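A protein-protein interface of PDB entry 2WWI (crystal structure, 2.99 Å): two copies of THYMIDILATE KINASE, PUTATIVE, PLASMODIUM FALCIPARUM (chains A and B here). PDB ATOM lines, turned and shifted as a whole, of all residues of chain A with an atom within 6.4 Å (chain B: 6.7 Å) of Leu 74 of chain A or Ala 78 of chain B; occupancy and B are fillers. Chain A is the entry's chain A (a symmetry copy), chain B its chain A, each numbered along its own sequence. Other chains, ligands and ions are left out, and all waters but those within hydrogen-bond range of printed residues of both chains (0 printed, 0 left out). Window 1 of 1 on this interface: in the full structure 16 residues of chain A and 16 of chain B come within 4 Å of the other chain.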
ATOM      1  N   ILE A  53     -16.165 -39.209  21.982  1.00  0.00           N
ATOM      2  CA  ILE A  53     -17.286 -38.281  21.963  1.00  0.00           C
ATOM      3  C   ILE A  53     -18.501 -38.957  21.384  1.00  0.00           C
ATOM      4  O   ILE A  53     -19.582 -38.940  21.986  1.00  0.00           O
ATOM      5  CB  ILE A  53     -16.916 -37.043  21.152  1.00  0.00           C
ATOM      6  CG1 ILE A  53     -15.690 -36.418  21.799  1.00  0.00           C
ATOM      7  CG2 ILE A  53     -18.045 -36.098  21.087  1.00  0.00           C
ATOM      8  CD1 ILE A  53     -15.344 -35.044  21.351  1.00  0.00           C
ATOM      9  N   SER A  68     -27.928 -32.003  29.161  1.00  0.00           N
ATOM     10  CA  SER A  68     -28.539 -30.735  28.807  1.00  0.00           C
ATOM     11  C   SER A  68     -28.383 -30.433  27.324  1.00  0.00           C
ATOM     12  O   SER A  68     -27.442 -30.879  26.657  1.00  0.00           O
ATOM     13  CB  SER A  68     -27.945 -29.601  29.614  1.00  0.00           C
ATOM     14  OG  SER A  68     -26.651 -29.296  29.133  1.00  0.00           O
ATOM     15  N   ASN A  69     -29.333 -29.653  26.838  1.00  0.00           N
ATOM     16  CA  ASN A  69     -29.357 -29.173  25.480  1.00  0.00           C
ATOM     17  C   ASN A  69     -28.030 -28.650  24.978  1.00  0.00           C
ATOM     18  O   ASN A  69     -27.541 -29.049  23.905  1.00  0.00           O
ATOM     19  CB  ASN A  69     -30.374 -28.071  25.401  1.00  0.00           C
ATOM     20  CG  ASN A  69     -31.768 -28.591  25.410  1.00  0.00           C
ATOM     21  OD1 ASN A  69     -32.703 -27.836  25.225  1.00  0.00           O
ATOM     22  ND2 ASN A  69     -31.928 -29.893  25.604  1.00  0.00           N
ATOM     23  N   GLU A  70     -27.440 -27.753  25.754  1.00  0.00           N
ATOM     24  CA  GLU A  70     -26.208 -27.133  25.320  1.00  0.00           C
ATOM     25  C   GLU A  70     -25.026 -28.092  25.366  1.00  0.00           C
ATOM     26  O   GLU A  70     -24.096 -27.962  24.588  1.00  0.00           O
ATOM     27  CB  GLU A  70     -25.951 -25.846  26.095  1.00  0.00           C
ATOM     28  CG  GLU A  70     -26.689 -25.810  27.402  1.00  0.00           C
ATOM     29  CD  GLU A  70     -27.956 -25.019  27.335  1.00  0.00           C
ATOM     30  OE1 GLU A  70     -27.939 -23.877  26.806  1.00  0.00           O
ATOM     31  OE2 GLU A  70     -28.970 -25.546  27.837  1.00  0.00           O
ATOM     32  N   THR A  71     -25.052 -29.078  26.240  1.00  0.00           N
ATOM     33  CA  THR A  71     -23.940 -30.036  26.237  1.00  0.00           C
ATOM     34  C   THR A  71     -23.901 -30.883  24.945  1.00  0.00           C
ATOM     35  O   THR A  71     -22.839 -31.010  24.305  1.00  0.00           O
ATOM     36  CB  THR A  71     -23.946 -30.949  27.454  1.00  0.00           C
ATOM     37  OG1 THR A  71     -24.298 -30.182  28.610  1.00  0.00           O
ATOM     38  CG2 THR A  71     -22.591 -31.507  27.650  1.00  0.00           C
ATOM     39  N   ILE A  72     -25.054 -31.453  24.574  1.00  0.00           N
ATOM     40  CA  ILE A  72     -25.113 -32.365  23.446  1.00  0.00           C
ATOM     41  C   ILE A  72     -24.820 -31.601  22.161  1.00  0.00           C
ATOM     42  O   ILE A  72     -24.012 -32.034  21.317  1.00  0.00           O
ATOM     43  CB  ILE A  72     -26.450 -33.097  23.382  1.00  0.00           C
ATOM     44  CG1 ILE A  72     -26.376 -34.236  22.379  1.00  0.00           C
ATOM     45  CG2 ILE A  72     -27.593 -32.164  23.026  1.00  0.00           C
ATOM     46  CD1 ILE A  72     -25.250 -35.197  22.622  1.00  0.00           C
ATOM     47  N   HIS A  73     -25.447 -30.433  22.033  1.00  0.00           N
ATOM     48  CA  HIS A  73     -25.092 -29.544  20.953  1.00  0.00           C
ATOM     49  C   HIS A  73     -23.558 -29.439  20.851  1.00  0.00           C
ATOM     50  O   HIS A  73     -22.978 -29.785  19.829  1.00  0.00           O
ATOM     51  CB  HIS A  73     -25.741 -28.164  21.085  1.00  0.00           C
ATOM     52  CG  HIS A  73     -25.447 -27.287  19.917  1.00  0.00           C
ATOM     53  ND1 HIS A  73     -26.181 -27.338  18.756  1.00  0.00           N
ATOM     54  CD2 HIS A  73     -24.451 -26.401  19.695  1.00  0.00           C
ATOM     55  CE1 HIS A  73     -25.666 -26.501  17.876  1.00  0.00           C
ATOM     56  NE2 HIS A  73     -24.619 -25.913  18.422  1.00  0.00           N
ATOM     57  N   LEU A  74     -22.907 -28.997  21.916  1.00  0.00           N
ATOM     58  CA  LEU A  74     -21.456 -28.839  21.889  1.00  0.00           C
ATOM     59  C   LEU A  74     -20.736 -30.136  21.523  1.00  0.00           C
ATOM     60  O   LEU A  74     -19.804 -30.127  20.739  1.00  0.00           O
ATOM     61  CB  LEU A  74     -20.953 -28.281  23.220  1.00  0.00           C
ATOM     62  CG  LEU A  74     -21.342 -26.820  23.457  1.00  0.00           C
ATOM     63  CD1 LEU A  74     -20.517 -26.281  24.633  1.00  0.00           C
ATOM     64  CD2 LEU A  74     -21.141 -25.961  22.182  1.00  0.00           C
ATOM     65  N   LEU A  75     -21.207 -31.250  22.069  1.00  0.00           N
ATOM     66  CA  LEU A  75     -20.646 -32.539  21.764  1.00  0.00           C
ATOM     67  C   LEU A  75     -20.718 -32.843  20.285  1.00  0.00           C
ATOM     68  O   LEU A  75     -19.784 -33.391  19.731  1.00  0.00           O
ATOM     69  CB  LEU A  75     -21.339 -33.628  22.570  1.00  0.00           C
ATOM     70  CG  LEU A  75     -20.628 -33.942  23.888  1.00  0.00           C
ATOM     71  CD1 LEU A  75     -20.667 -35.435  24.182  1.00  0.00           C
ATOM     72  CD2 LEU A  75     -19.201 -33.509  23.796  1.00  0.00           C
ATOM     73  N   PHE A  76     -21.814 -32.464  19.643  1.00  0.00           N
ATOM     74  CA  PHE A  76     -21.959 -32.702  18.219  1.00  0.00           C
ATOM     75  C   PHE A  76     -20.937 -31.943  17.417  1.00  0.00           C
ATOM     76  O   PHE A  76     -20.320 -32.480  16.509  1.00  0.00           O
ATOM     77  CB  PHE A  76     -23.344 -32.324  17.742  1.00  0.00           C
ATOM     78  CG  PHE A  76     -24.305 -33.459  17.739  1.00  0.00           C
ATOM     79  CD1 PHE A  76     -24.138 -34.524  16.853  1.00  0.00           C
ATOM     80  CD2 PHE A  76     -25.390 -33.468  18.601  1.00  0.00           C
ATOM     81  CE1 PHE A  76     -25.041 -35.593  16.835  1.00  0.00           C
ATOM     82  CE2 PHE A  76     -26.307 -34.533  18.584  1.00  0.00           C
ATOM     83  CZ  PHE A  76     -26.127 -35.598  17.698  1.00  0.00           C
ATOM     84  N   SER A  77     -20.762 -30.680  17.748  1.00  0.00           N
ATOM     85  CA  SER A  77     -19.821 -29.841  17.037  1.00  0.00           C
ATOM     86  C   SER A  77     -18.392 -30.372  17.194  1.00  0.00           C
ATOM     87  O   SER A  77     -17.719 -30.656  16.217  1.00  0.00           O
ATOM     88  CB  SER A  77     -19.937 -28.438  17.571  1.00  0.00           C
ATOM     89  OG  SER A  77     -19.065 -27.603  16.874  1.00  0.00           O
ATOM     90  N   ALA A  78     -17.947 -30.516  18.437  1.00  0.00           N
ATOM     91  CA  ALA A  78     -16.697 -31.195  18.757  1.00  0.00           C
ATOM     92  C   ALA A  78     -16.421 -32.399  17.882  1.00  0.00           C
ATOM     93  O   ALA A  78     -15.343 -32.517  17.346  1.00  0.00           O
ATOM     94  CB  ALA A  78     -16.698 -31.616  20.187  1.00  0.00           C
ATOM     95  N   ASN A  79     -17.397 -33.289  17.763  1.00  0.00           N
ATOM     96  CA  ASN A  79     -17.298 -34.465  16.928  1.00  0.00           C
ATOM     97  C   ASN A  79     -16.894 -34.183  15.451  1.00  0.00           C
ATOM     98  O   ASN A  79     -16.137 -34.956  14.813  1.00  0.00           O
ATOM     99  CB  ASN A  79     -18.645 -35.170  16.942  1.00  0.00           C
ATOM    100  CG  ASN A  79     -18.564 -36.612  16.467  1.00  0.00           C
ATOM    101  OD1 ASN A  79     -19.443 -37.097  15.750  1.00  0.00           O
ATOM    102  ND2 ASN A  79     -17.496 -37.307  16.872  1.00  0.00           N
ATOM    103  N   TRP A 120     -26.059 -18.882  18.534  1.00  0.00           N
ATOM    104  CA  TRP A 120     -25.387 -19.698  19.530  1.00  0.00           C
ATOM    105  C   TRP A 120     -24.952 -21.046  18.954  1.00  0.00           C
ATOM    106  O   TRP A 120     -23.786 -21.427  19.126  1.00  0.00           O
ATOM    107  CB  TRP A 120     -26.257 -19.897  20.773  1.00  0.00           C
ATOM    108  CG  TRP A 120     -25.404 -20.292  21.899  1.00  0.00           C
ATOM    109  CD1 TRP A 120     -24.691 -19.470  22.695  1.00  0.00           C
ATOM    110  CD2 TRP A 120     -25.099 -21.625  22.319  1.00  0.00           C
ATOM    111  NE1 TRP A 120     -23.982 -20.193  23.612  1.00  0.00           N
ATOM    112  CE2 TRP A 120     -24.210 -21.524  23.399  1.00  0.00           C
ATOM    113  CE3 TRP A 120     -25.501 -22.900  21.889  1.00  0.00           C
ATOM    114  CZ2 TRP A 120     -23.703 -22.648  24.067  1.00  0.00           C
ATOM    115  CZ3 TRP A 120     -25.003 -24.022  22.558  1.00  0.00           C
ATOM    116  CH2 TRP A 120     -24.112 -23.883  23.637  1.00  0.00           C
ATOM    117  N   PRO A 124     -19.976 -22.582  17.427  1.00  0.00           N
ATOM    118  CA  PRO A 124     -18.922 -23.556  17.590  1.00  0.00           C
ATOM    119  C   PRO A 124     -18.494 -24.289  16.298  1.00  0.00           C
ATOM    120  O   PRO A 124     -17.355 -24.731  16.228  1.00  0.00           O
ATOM    121  CB  PRO A 124     -19.525 -24.522  18.597  1.00  0.00           C
ATOM    122  CG  PRO A 124     -20.963 -24.475  18.303  1.00  0.00           C
ATOM    123  CD  PRO A 124     -21.244 -23.064  17.981  1.00  0.00           C
ATOM    124  N   ILE B  53     -17.282 -36.811  29.550  1.00  0.00           N
ATOM    125  CA  ILE B  53     -16.484 -35.780  28.902  1.00  0.00           C
ATOM    126  C   ILE B  53     -15.187 -35.591  29.647  1.00  0.00           C
ATOM    127  O   ILE B  53     -14.104 -35.626  29.050  1.00  0.00           O
ATOM    128  CB  ILE B  53     -17.273 -34.477  28.845  1.00  0.00           C
ATOM    129  CG1 ILE B  53     -18.557 -34.747  28.078  1.00  0.00           C
ATOM    130  CG2 ILE B  53     -16.476 -33.406  28.222  1.00  0.00           C
ATOM    131  CD1 ILE B  53     -19.326 -33.551  27.649  1.00  0.00           C
ATOM    132  N   ILE B  57     -11.328 -35.217  28.723  1.00  0.00           N
ATOM    133  CA  ILE B  57     -10.504 -34.051  29.006  1.00  0.00           C
ATOM    134  C   ILE B  57      -9.262 -34.515  29.768  1.00  0.00           C
ATOM    135  O   ILE B  57      -8.129 -34.009  29.555  1.00  0.00           O
ATOM    136  CB  ILE B  57     -11.252 -32.955  29.778  1.00  0.00           C
ATOM    137  CG1 ILE B  57     -12.503 -32.515  28.992  1.00  0.00           C
ATOM    138  CG2 ILE B  57     -10.312 -31.800  30.046  1.00  0.00           C
ATOM    139  CD1 ILE B  57     -13.160 -31.213  29.453  1.00  0.00           C
ATOM    140  N   HIS B  73     -10.966 -27.593  23.359  1.00  0.00           N
ATOM    141  CA  HIS B  73     -11.667 -26.385  23.724  1.00  0.00           C
ATOM    142  C   HIS B  73     -13.168 -26.688  23.894  1.00  0.00           C
ATOM    143  O   HIS B  73     -13.721 -26.505  24.972  1.00  0.00           O
ATOM    144  CB  HIS B  73     -11.433 -25.243  22.732  1.00  0.00           C
ATOM    145  CG  HIS B  73     -12.080 -23.974  23.167  1.00  0.00           C
ATOM    146  ND1 HIS B  73     -11.480 -23.109  24.050  1.00  0.00           N
ATOM    147  CD2 HIS B  73     -13.306 -23.465  22.914  1.00  0.00           C
ATOM    148  CE1 HIS B  73     -12.299 -22.105  24.302  1.00  0.00           C
ATOM    149  NE2 HIS B  73     -13.413 -22.293  23.620  1.00  0.00           N
ATOM    150  N   LEU B  74     -13.810 -27.181  22.846  1.00  0.00           N
ATOM    151  CA  LEU B  74     -15.241 -27.464  22.916  1.00  0.00           C
ATOM    152  C   LEU B  74     -15.589 -28.425  24.052  1.00  0.00           C
ATOM    153  O   LEU B  74     -16.556 -28.218  24.763  1.00  0.00           O
ATOM    154  CB  LEU B  74     -15.749 -27.986  21.572  1.00  0.00           C
ATOM    155  CG  LEU B  74     -15.777 -26.921  20.473  1.00  0.00           C
ATOM    156  CD1 LEU B  74     -16.602 -27.456  19.296  1.00  0.00           C
ATOM    157  CD2 LEU B  74     -16.341 -25.574  20.996  1.00  0.00           C
ATOM    158  N   LEU B  75     -14.764 -29.449  24.236  1.00  0.00           N
ATOM    159  CA  LEU B  75     -14.957 -30.394  25.303  1.00  0.00           C
ATOM    160  C   LEU B  75     -14.947 -29.718  26.655  1.00  0.00           C
ATOM    161  O   LEU B  75     -15.733 -30.067  27.515  1.00  0.00           O
ATOM    162  CB  LEU B  75     -13.904 -31.490  25.243  1.00  0.00           C
ATOM    163  CG  LEU B  75     -14.362 -32.717  24.451  1.00  0.00           C
ATOM    164  CD1 LEU B  75     -13.865 -33.999  25.104  1.00  0.00           C
ATOM    165  CD2 LEU B  75     -15.855 -32.749  24.406  1.00  0.00           C
ATOM    166  N   PHE B  76     -14.076 -28.735  26.833  1.00  0.00           N
ATOM    167  CA  PHE B  76     -14.009 -28.023  28.094  1.00  0.00           C
ATOM    168  C   PHE B  76     -15.280 -27.269  28.381  1.00  0.00           C
ATOM    169  O   PHE B  76     -15.803 -27.308  29.485  1.00  0.00           O
ATOM    170  CB  PHE B  76     -12.846 -27.055  28.112  1.00  0.00           C
ATOM    171  CG  PHE B  76     -11.603 -27.626  28.698  1.00  0.00           C
ATOM    172  CD1 PHE B  76     -11.543 -27.943  30.054  1.00  0.00           C
ATOM    173  CD2 PHE B  76     -10.483 -27.835  27.909  1.00  0.00           C
ATOM    174  CE1 PHE B  76     -10.377 -28.472  30.618  1.00  0.00           C
ATOM    175  CE2 PHE B  76      -9.304 -28.358  28.469  1.00  0.00           C
ATOM    176  CZ  PHE B  76      -9.255 -28.678  29.827  1.00  0.00           C
ATOM    177  N   SER B  77     -15.778 -26.572  27.380  1.00  0.00           N
ATOM    178  CA  SER B  77     -16.986 -25.790  27.539  1.00  0.00           C
ATOM    179  C   SER B  77     -18.179 -26.694  27.871  1.00  0.00           C
ATOM    180  O   SER B  77     -18.834 -26.517  28.885  1.00  0.00           O
ATOM    181  CB  SER B  77     -17.228 -25.025  26.264  1.00  0.00           C
ATOM    182  OG  SER B  77     -18.368 -24.235  26.407  1.00  0.00           O
ATOM    183  N   ALA B  78     -18.439 -27.672  27.011  1.00  0.00           N
ATOM    184  CA  ALA B  78     -19.403 -28.731  27.284  1.00  0.00           C
ATOM    185  C   ALA B  78     -19.404 -29.191  28.727  1.00  0.00           C
ATOM    186  O   ALA B  78     -20.450 -29.269  29.330  1.00  0.00           O
ATOM    187  CB  ALA B  78     -19.139 -29.899  26.397  1.00  0.00           C
ATOM    188  N   ASN B  79     -18.230 -29.504  29.256  1.00  0.00           N
ATOM    189  CA  ASN B  79     -18.067 -29.915  30.633  1.00  0.00           C
ATOM    190  C   ASN B  79     -18.679 -28.938  31.680  1.00  0.00           C
ATOM    191  O   ASN B  79     -19.239 -29.355  32.724  1.00  0.00           O
ATOM    192  CB  ASN B  79     -16.579 -30.063  30.910  1.00  0.00           C
ATOM    193  CG  ASN B  79     -16.288 -30.883  32.157  1.00  0.00           C
ATOM    194  OD1 ASN B  79     -15.381 -30.565  32.931  1.00  0.00           O
ATOM    195  ND2 ASN B  79     -17.064 -31.953  32.354  1.00  0.00           N
ATOM    196  N   ARG B  80     -18.549 -27.642  31.422  1.00  0.00           N
ATOM    197  CA  ARG B  80     -19.130 -26.655  32.302  1.00  0.00           C
ATOM    198  C   ARG B  80     -20.615 -26.681  32.145  1.00  0.00           C
ATOM    199  O   ARG B  80     -21.331 -26.592  33.118  1.00  0.00           O
ATOM    200  CB  ARG B  80     -18.604 -25.269  31.988  1.00  0.00           C
ATOM    201  CG  ARG B  80     -17.250 -25.037  32.539  1.00  0.00           C
ATOM    202  CD  ARG B  80     -16.836 -23.638  32.289  1.00  0.00           C
ATOM    203  NE  ARG B  80     -16.351 -23.399  30.925  1.00  0.00           N
ATOM    204  CZ  ARG B  80     -15.240 -23.925  30.409  1.00  0.00           C
ATOM    205  NH1 ARG B  80     -14.508 -24.795  31.102  1.00  0.00           N
ATOM    206  NH2 ARG B  80     -14.874 -23.595  29.183  1.00  0.00           N
ATOM    207  N   TRP B  81     -21.084 -26.809  30.915  1.00  0.00           N
ATOM    208  CA  TRP B  81     -22.519 -26.833  30.672  1.00  0.00           C
ATOM    209  C   TRP B  81     -23.197 -28.006  31.378  1.00  0.00           C
ATOM    210  O   TRP B  81     -24.339 -27.872  31.792  1.00  0.00           O
ATOM    211  CB  TRP B  81     -22.840 -26.836  29.180  1.00  0.00           C
ATOM    212  CG  TRP B  81     -22.788 -25.457  28.526  1.00  0.00           C
ATOM    213  CD1 TRP B  81     -21.778 -24.941  27.713  1.00  0.00           C
ATOM    214  CD2 TRP B  81     -23.791 -24.434  28.604  1.00  0.00           C
ATOM    215  NE1 TRP B  81     -22.115 -23.659  27.304  1.00  0.00           N
ATOM    216  CE2 TRP B  81     -23.339 -23.333  27.832  1.00  0.00           C
ATOM    217  CE3 TRP B  81     -25.021 -24.335  29.262  1.00  0.00           C
ATOM    218  CZ2 TRP B  81     -24.075 -22.161  27.712  1.00  0.00           C
ATOM    219  CZ3 TRP B  81     -25.770 -23.153  29.114  1.00  0.00           C
ATOM    220  CH2 TRP B  81     -25.288 -22.096  28.354  1.00  0.00           C
ATOM    221  N   GLU B  82     -22.512 -29.137  31.563  1.00  0.00           N
ATOM    222  CA  GLU B  82     -23.171 -30.260  32.251  1.00  0.00           C
ATOM    223  C   GLU B  82     -23.296 -30.063  33.786  1.00  0.00           C
ATOM    224  O   GLU B  82     -23.856 -30.889  34.483  1.00  0.00           O
ATOM    225  CB  GLU B  82     -22.597 -31.621  31.850  1.00  0.00           C
ATOM    226  CG  GLU B  82     -21.113 -31.812  32.106  1.00  0.00           C
ATOM    227  CD  GLU B  82     -20.632 -33.217  31.745  1.00  0.00           C
ATOM    228  OE1 GLU B  82     -21.493 -34.134  31.626  1.00  0.00           O
ATOM    229  OE2 GLU B  82     -19.398 -33.384  31.589  1.00  0.00           O
ATOM    230  N   HIS B  83     -22.811 -28.923  34.269  1.00  0.00           N
ATOM    231  CA  HIS B  83     -22.920 -28.533  35.658  1.00  0.00           C
ATOM    232  C   HIS B  83     -23.805 -27.312  35.910  1.00  0.00           C
ATOM    233  O   HIS B  83     -24.126 -27.006  37.069  1.00  0.00           O
ATOM    234  CB  HIS B  83     -21.549 -28.269  36.199  1.00  0.00           C
ATOM    235  CG  HIS B  83     -20.711 -29.494  36.284  1.00  0.00           C
ATOM    236  ND1 HIS B  83     -20.097 -30.049  35.181  1.00  0.00           N
ATOM    237  CD2 HIS B  83     -20.386 -30.277  37.339  1.00  0.00           C
ATOM    238  CE1 HIS B  83     -19.428 -31.124  35.555  1.00  0.00           C
ATOM    239  NE2 HIS B  83     -19.585 -31.282  36.859  1.00  0.00           N
ATOM    240  N   PRO B 124     -18.893 -20.543  22.880  1.00  0.00           N
ATOM    241  CA  PRO B 124     -19.600 -21.673  23.436  1.00  0.00           C
ATOM    242  C   PRO B 124     -19.923 -21.574  24.944  1.00  0.00           C
ATOM    243  O   PRO B 124     -20.888 -22.192  25.375  1.00  0.00           O
ATOM    244  CB  PRO B 124     -18.648 -22.823  23.151  1.00  0.00           C
ATOM    245  CG  PRO B 124     -17.321 -22.199  23.216  1.00  0.00           C
ATOM    246  CD  PRO B 124     -17.491 -20.869  22.602  1.00  0.00           C
ATOM    247  N   ASP B 125     -19.124 -20.834  25.721  1.00  0.00           N
ATOM    248  CA  ASP B 125     -19.356 -20.664  27.158  1.00  0.00           C
ATOM    249  C   ASP B 125     -20.367 -19.537  27.355  1.00  0.00           C
ATOM    250  O   ASP B 125     -21.015 -19.448  28.402  1.00  0.00           O
ATOM    251  CB  ASP B 125     -18.083 -20.271  27.896  1.00  0.00           C
ATOM    252  CG  ASP B 125     -17.167 -21.445  28.215  1.00  0.00           C
ATOM    253  OD1 ASP B 125     -17.629 -22.599  28.422  1.00  0.00           O
ATOM    254  OD2 ASP B 125     -15.942 -21.186  28.295  1.00  0.00           O
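O of Pro 124 of chain B sits at hydrogen-bond distance from OG of Ser 77 of chain B (3.4 Å).
OD1 of Asp 125 of chain B sits at hydrogen-bond distance from OG of Ser 77 of chain B, 2.7 Å away.
ND2 of Asn 79 of chain B is in hydrogen-bond range of OE2 of Glu 82 of chain B (2.8 Å).
The backbone carbonyl oxygen (O) of Pro 124 of chain B is in hydrogen-bond range of the indole nitrogen (NE1) of Trp 81 of chain B (2.7 Å).
The side-chain hydroxyl (OG) of Ser 68 of chain A is in hydrogen-bond range of the side-chain hydroxyl (OG1) of Thr 71 of chain A, at 2.6 Å.
The backbone carbonyl oxygen (O) of Pro 124 of chain A is in hydrogen-bond range of the side-chain hydroxyl (OG) of Ser 77 of chain A (3.4 Å).
Ile 53 of chain A touches Leu 75 of chain B.
Ser 68 of chain A touches Trp 81 of chain B.
Glu 70 of chain A touches Trp 81 of chain B (CG to CE3, 2.9 Å).
Ile 53 of chain B touches Thr 71 of chain A.
Thr 71 of chain A touches Ala 78 of chain B (CG2 to O, 3.5 Å).
Thr 71 of chain A touches Glu 82 of chain B.
Trp 81 of chain B touches Leu 74 of chain A (CD1 to CD1, 3.6 Å).
CD2 of Leu 75 of chain B touches CD2 of Leu 75 of chain A, at 3.5 Å.
CD1 of Leu 74 of chain B touches OG of Ser 77 of chain A, 3.5 Å away.
Trp 120 of chain A touches Pro 124 of chain B (CZ2 to O, 3.1 Å).
Leu 74 of chain A touches three residues of chain B.
Pro 124 of chain A touches none of the printed residues of chain B.
Printed residues of chain A within 4 Å of Ser 77 of chain B: Leu 74 (3.5 Å).
Of chain A, only Thr 71 (3.5 Å) and Leu 74 (3.5 Å) come within 4 Å of Ala 78 of chain B.
Printed residues of chain A within 4 Å of Glu 82 of chain B: Thr 71.
The nearest residue of chain B that does not touch Leu 74 of chain A is Pro 124 of chain B (4.1 Å).
The nearest printed residue of chain B that does not touch Ser 68 of chain A is Glu 82 of chain B (4.8 Å).
Hydrophobic or aromatic side chains of chain A within 4 Å of the printed part of chain B: Ile 53, Leu 74, Leu 75, Ala 78 and Trp 120.
Printed residues of chain B that touch a printed residue of chain A: Ile 53, Leu 74, Leu 75, Ser 77, Ala 78, Trp 81, Glu 82 and Pro 124.
Among the printed residues, 16 pairs touch across the chains.
Among the printed residues, no Asp or Glu carboxylate lies within 4 Å of a Lys or Arg side-chain nitrogen of the other chain.
Ile 53 of chain A touches Leu 75 of chain B, and with the chains exchanged Leu 75 of chain A touches Ile 53 of chain B.
Leu 74 of chain A touches Ser 77 of chain B, and with the chains exchanged Ser 77 of chain A touches Leu 74 of chain B.
Leu 74 of chain A touches Ala 78 of chain B, and with the chains exchanged Ala 78 of chain A touches Leu 74 of chain B.
Leu 75 of chain A touches its own counterpart, Leu 75 of chain B.
Of the 16 pairs that touch across the chains among the printed residues, 7 have their exchanged pair printed and touching as well.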
